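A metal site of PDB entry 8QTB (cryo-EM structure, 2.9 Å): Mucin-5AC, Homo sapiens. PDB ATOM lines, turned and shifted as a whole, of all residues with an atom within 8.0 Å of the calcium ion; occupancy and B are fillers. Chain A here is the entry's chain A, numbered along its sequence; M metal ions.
The side-chain carboxylate (OD1) of Asp 263 binds the calcium ion, 2.4 Å away. The calcium ion is bound by OD1 of Asp 269. The calcium ion is bound by OD1 of Asn 268, at 2.4 Å. O of Ile 265 is bound to the calcium ion (2.4 Å). The side-chain amide oxygen (OD1) of Asn 261 is bound to the calcium ion, at 2.4 Å. The side-chain carboxylate (OD2) of Asp 138 is bound to the calcium ion (2.9 Å). The calcium ion has six donor atoms within binding distance. Slightly farther from the calcium ion lies OD2 of Asp 263 (3.1 Å).
The nearest printed residue that does not touch the calcium ion is Ala 266 (4.6 Å).
OG1 of Thr 136 sits at hydrogen-bond distance from OD2 of Asp 269, at 3.1 Å. OD1 of Asp 138 is in hydrogen-bond range of N of Asp 264, 3.0 Å away.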
ATOM      1  N   THR A 136      15.096   0.058  15.011  1.00  0.00           N
ATOM      2  CA  THR A 136      15.977  -0.991  14.517  1.00  0.00           C
ATOM      3  C   THR A 136      15.278  -2.340  14.544  1.00  0.00           C
ATOM      4  O   THR A 136      14.207  -2.522  15.134  1.00  0.00           O
ATOM      5  CB  THR A 136      17.257  -1.044  15.343  1.00  0.00           C
ATOM      6  OG1 THR A 136      16.960  -1.538  16.662  1.00  0.00           O
ATOM      7  CG2 THR A 136      17.882   0.339  15.456  1.00  0.00           C
ATOM      8  N   PHE A 137      15.894  -3.311  13.865  1.00  0.00           N
ATOM      9  CA  PHE A 137      15.367  -4.672  13.869  1.00  0.00           C
ATOM     10  C   PHE A 137      15.350  -5.257  15.270  1.00  0.00           C
ATOM     11  O   PHE A 137      14.387  -5.920  15.674  1.00  0.00           O
ATOM     12  CB  PHE A 137      16.185  -5.559  12.930  1.00  0.00           C
ATOM     13  CG  PHE A 137      15.825  -5.401  11.474  1.00  0.00           C
ATOM     14  CD1 PHE A 137      14.582  -5.784  11.012  1.00  0.00           C
ATOM     15  CD2 PHE A 137      16.745  -4.875  10.579  1.00  0.00           C
ATOM     16  CE1 PHE A 137      14.257  -5.633   9.675  1.00  0.00           C
ATOM     17  CE2 PHE A 137      16.426  -4.732   9.245  1.00  0.00           C
ATOM     18  CZ  PHE A 137      15.179  -5.114   8.792  1.00  0.00           C
ATOM     19  N   ASP A 138      16.421  -5.040  16.032  1.00  0.00           N
ATOM     20  CA  ASP A 138      16.508  -5.583  17.384  1.00  0.00           C
ATOM     21  C   ASP A 138      15.510  -4.897  18.316  1.00  0.00           C
ATOM     22  O   ASP A 138      14.945  -5.552  19.198  1.00  0.00           O
ATOM     23  CB  ASP A 138      17.937  -5.449  17.907  1.00  0.00           C
ATOM     24  CG  ASP A 138      18.950  -6.064  16.969  1.00  0.00           C
ATOM     25  OD1 ASP A 138      18.578  -6.957  16.190  1.00  0.00           O
ATOM     26  OD2 ASP A 138      20.129  -5.638  17.013  1.00  0.00           O
ATOM     27  N   GLY A 139      15.285  -3.600  18.138  1.00  0.00           N
ATOM     28  CA  GLY A 139      14.311  -2.898  18.946  1.00  0.00           C
ATOM     29  C   GLY A 139      14.744  -1.517  19.400  1.00  0.00           C
ATOM     30  O   GLY A 139      13.982  -0.812  20.059  1.00  0.00           O
ATOM     31  N   GLN A 140      15.962  -1.116  19.048  1.00  0.00           N
ATOM     32  CA  GLN A 140      16.458   0.192  19.446  1.00  0.00           C
ATOM     33  C   GLN A 140      15.692   1.292  18.713  1.00  0.00           C
ATOM     34  O   GLN A 140      15.385   1.174  17.532  1.00  0.00           O
ATOM     35  CB  GLN A 140      17.950   0.310  19.157  1.00  0.00           C
ATOM     36  CG  GLN A 140      18.576   1.624  19.612  1.00  0.00           C
ATOM     37  CD  GLN A 140      18.666   1.740  21.121  1.00  0.00           C
ATOM     38  OE1 GLN A 140      18.681   0.733  21.833  1.00  0.00           O
ATOM     39  NE2 GLN A 140      18.709   2.967  21.615  1.00  0.00           N
ATOM     40  N   CYS A 259      19.384   0.454  10.041  1.00  0.00           N
ATOM     41  CA  CYS A 259      18.601  -0.477  10.843  1.00  0.00           C
ATOM     42  C   CYS A 259      19.457  -1.302  11.794  1.00  0.00           C
ATOM     43  O   CYS A 259      18.913  -1.941  12.697  1.00  0.00           O
ATOM     44  CB  CYS A 259      17.797  -1.405   9.931  1.00  0.00           C
ATOM     45  SG  CYS A 259      16.486  -0.594   8.982  1.00  0.00           S
ATOM     46  N   GLY A 260      20.773  -1.310  11.610  1.00  0.00           N
ATOM     47  CA  GLY A 260      21.660  -2.039  12.494  1.00  0.00           C
ATOM     48  C   GLY A 260      21.767  -3.505  12.143  1.00  0.00           C
ATOM     49  O   GLY A 260      20.979  -4.065  11.372  1.00  0.00           O
ATOM     50  N   ASN A 261      22.779  -4.147  12.717  1.00  0.00           N
ATOM     51  CA  ASN A 261      22.985  -5.570  12.496  1.00  0.00           C
ATOM     52  C   ASN A 261      21.872  -6.386  13.155  1.00  0.00           C
ATOM     53  O   ASN A 261      21.419  -6.059  14.249  1.00  0.00           O
ATOM     54  CB  ASN A 261      24.350  -6.011  13.019  1.00  0.00           C
ATOM     55  CG  ASN A 261      24.563  -5.620  14.468  1.00  0.00           C
ATOM     56  OD1 ASN A 261      23.831  -4.799  15.015  1.00  0.00           O
ATOM     57  ND2 ASN A 261      25.581  -6.203  15.088  1.00  0.00           N
ATOM     58  N   PHE A 262      21.438  -7.439  12.463  1.00  0.00           N
ATOM     59  CA  PHE A 262      20.354  -8.291  12.947  1.00  0.00           C
ATOM     60  C   PHE A 262      20.902  -9.370  13.883  1.00  0.00           C
ATOM     61  O   PHE A 262      20.767 -10.573  13.656  1.00  0.00           O
ATOM     62  CB  PHE A 262      19.599  -8.898  11.777  1.00  0.00           C
ATOM     63  CG  PHE A 262      18.312  -9.567  12.161  1.00  0.00           C
ATOM     64  CD1 PHE A 262      17.641  -9.219  13.321  1.00  0.00           C
ATOM     65  CD2 PHE A 262      17.768 -10.549  11.352  1.00  0.00           C
ATOM     66  CE1 PHE A 262      16.459  -9.838  13.667  1.00  0.00           C
ATOM     67  CE2 PHE A 262      16.581 -11.176  11.695  1.00  0.00           C
ATOM     68  CZ  PHE A 262      15.932 -10.820  12.855  1.00  0.00           C
ATOM     69  N   ASP A 263      21.547  -8.919  14.956  1.00  0.00           N
ATOM     70  CA  ASP A 263      22.136  -9.810  15.951  1.00  0.00           C
ATOM     71  C   ASP A 263      21.291  -9.928  17.208  1.00  0.00           C
ATOM     72  O   ASP A 263      21.723 -10.568  18.179  1.00  0.00           O
ATOM     73  CB  ASP A 263      23.541  -9.323  16.324  1.00  0.00           C
ATOM     74  CG  ASP A 263      23.561  -7.903  16.832  1.00  0.00           C
ATOM     75  OD1 ASP A 263      22.540  -7.199  16.669  1.00  0.00           O
ATOM     76  OD2 ASP A 263      24.595  -7.477  17.387  1.00  0.00           O
ATOM     77  N   ASP A 264      20.091  -9.346  17.215  1.00  0.00           N
ATOM     78  CA  ASP A 264      19.177  -9.378  18.366  1.00  0.00           C
ATOM     79  C   ASP A 264      19.791  -8.735  19.607  1.00  0.00           C
ATOM     80  O   ASP A 264      19.443  -9.098  20.737  1.00  0.00           O
ATOM     81  CB  ASP A 264      18.728 -10.815  18.672  1.00  0.00           C
ATOM     82  CG  ASP A 264      17.878 -11.413  17.577  1.00  0.00           C
ATOM     83  OD1 ASP A 264      17.416 -10.648  16.699  1.00  0.00           O
ATOM     84  OD2 ASP A 264      17.664 -12.641  17.581  1.00  0.00           O
ATOM     85  N   ILE A 265      20.704  -7.787  19.414  1.00  0.00           N
ATOM     86  CA  ILE A 265      21.325  -7.052  20.509  1.00  0.00           C
ATOM     87  C   ILE A 265      21.142  -5.568  20.221  1.00  0.00           C
ATOM     88  O   ILE A 265      21.652  -5.054  19.226  1.00  0.00           O
ATOM     89  CB  ILE A 265      22.809  -7.394  20.673  1.00  0.00           C
ATOM     90  CG1 ILE A 265      23.030  -8.902  20.598  1.00  0.00           C
ATOM     91  CG2 ILE A 265      23.331  -6.862  22.006  1.00  0.00           C
ATOM     92  CD1 ILE A 265      24.486  -9.309  20.604  1.00  0.00           C
ATOM     93  N   ALA A 266      20.417  -4.873  21.103  1.00  0.00           N
ATOM     94  CA  ALA A 266      20.084  -3.473  20.864  1.00  0.00           C
ATOM     95  C   ALA A 266      21.253  -2.542  21.131  1.00  0.00           C
ATOM     96  O   ALA A 266      21.356  -1.495  20.479  1.00  0.00           O
ATOM     97  CB  ALA A 266      18.887  -3.071  21.726  1.00  0.00           C
ATOM     98  N   VAL A 267      22.133  -2.878  22.075  1.00  0.00           N
ATOM     99  CA  VAL A 267      23.176  -1.949  22.480  1.00  0.00           C
ATOM    100  C   VAL A 267      24.186  -1.702  21.372  1.00  0.00           C
ATOM    101  O   VAL A 267      24.702  -0.588  21.225  1.00  0.00           O
ATOM    102  CB  VAL A 267      23.866  -2.443  23.771  1.00  0.00           C
ATOM    103  CG1 VAL A 267      22.865  -2.469  24.921  1.00  0.00           C
ATOM    104  CG2 VAL A 267      24.476  -3.816  23.566  1.00  0.00           C
ATOM    105  N   ASN A 268      24.494  -2.719  20.567  1.00  0.00           N
ATOM    106  CA  ASN A 268      25.527  -2.616  19.533  1.00  0.00           C
ATOM    107  C   ASN A 268      24.932  -2.359  18.154  1.00  0.00           C
ATOM    108  O   ASN A 268      25.451  -2.858  17.146  1.00  0.00           O
ATOM    109  CB  ASN A 268      26.384  -3.876  19.520  1.00  0.00           C
ATOM    110  CG  ASN A 268      25.567  -5.146  19.460  1.00  0.00           C
ATOM    111  OD1 ASN A 268      24.423  -5.144  19.023  1.00  0.00           O
ATOM    112  ND2 ASN A 268      26.160  -6.247  19.912  1.00  0.00           N
ATOM    113  N   ASP A 269      23.864  -1.566  18.075  1.00  0.00           N
ATOM    114  CA  ASP A 269      23.231  -1.227  16.809  1.00  0.00           C
ATOM    115  C   ASP A 269      23.749   0.086  16.227  1.00  0.00           C
ATOM    116  O   ASP A 269      23.220   0.552  15.212  1.00  0.00           O
ATOM    117  CB  ASP A 269      21.715  -1.152  16.976  1.00  0.00           C
ATOM    118  CG  ASP A 269      21.025  -2.466  16.691  1.00  0.00           C
ATOM    119  OD1 ASP A 269      21.648  -3.329  16.033  1.00  0.00           O
ATOM    120  OD2 ASP A 269      19.866  -2.643  17.110  1.00  0.00           O
ATOM    121  N   PHE A 270      24.765   0.684  16.833  1.00  0.00           N
ATOM    122  CA  PHE A 270      25.279   1.983  16.429  1.00  0.00           C
ATOM    123  C   PHE A 270      26.628   1.881  15.725  1.00  0.00           C
ATOM    124  O   PHE A 270      27.514   2.712  15.917  1.00  0.00           O
ATOM    125  CB  PHE A 270      25.382   2.920  17.631  1.00  0.00           C
ATOM    126  CG  PHE A 270      24.073   3.533  18.032  1.00  0.00           C
ATOM    127  CD1 PHE A 270      22.953   3.419  17.218  1.00  0.00           C
ATOM    128  CD2 PHE A 270      23.957   4.218  19.231  1.00  0.00           C
ATOM    129  CE1 PHE A 270      21.746   3.982  17.595  1.00  0.00           C
ATOM    130  CE2 PHE A 270      22.750   4.782  19.608  1.00  0.00           C
ATOM    131  CZ  PHE A 270      21.642   4.660  18.788  1.00  0.00           C
ATOM    132  N   ALA A 271      26.800   0.847  14.907  1.00  0.00           N
ATOM    133  CA  ALA A 271      28.044   0.690  14.150  1.00  0.00           C
ATOM    134  C   ALA A 271      28.156   1.790  13.106  1.00  0.00           C
ATOM    135  O   ALA A 271      27.238   1.983  12.294  1.00  0.00           O
ATOM    136  CB  ALA A 271      28.103  -0.685  13.501  1.00  0.00           C
ATOM    137  N   VAL A 277      31.100   0.763  17.428  1.00  0.00           N
ATOM    138  CA  VAL A 277      29.906   1.352  18.024  1.00  0.00           C
ATOM    139  C   VAL A 277      30.267   2.704  18.634  1.00  0.00           C
ATOM    140  O   VAL A 277      31.217   2.813  19.405  1.00  0.00           O
ATOM    141  CB  VAL A 277      29.292   0.422  19.083  1.00  0.00           C
ATOM    142  CG1 VAL A 277      28.435  -0.637  18.408  1.00  0.00           C
ATOM    143  CG2 VAL A 277      30.380  -0.235  19.911  1.00  0.00           C
HETATM  144 CA    CA M   1      22.906  -4.937  17.212  1.00  0.00          CA
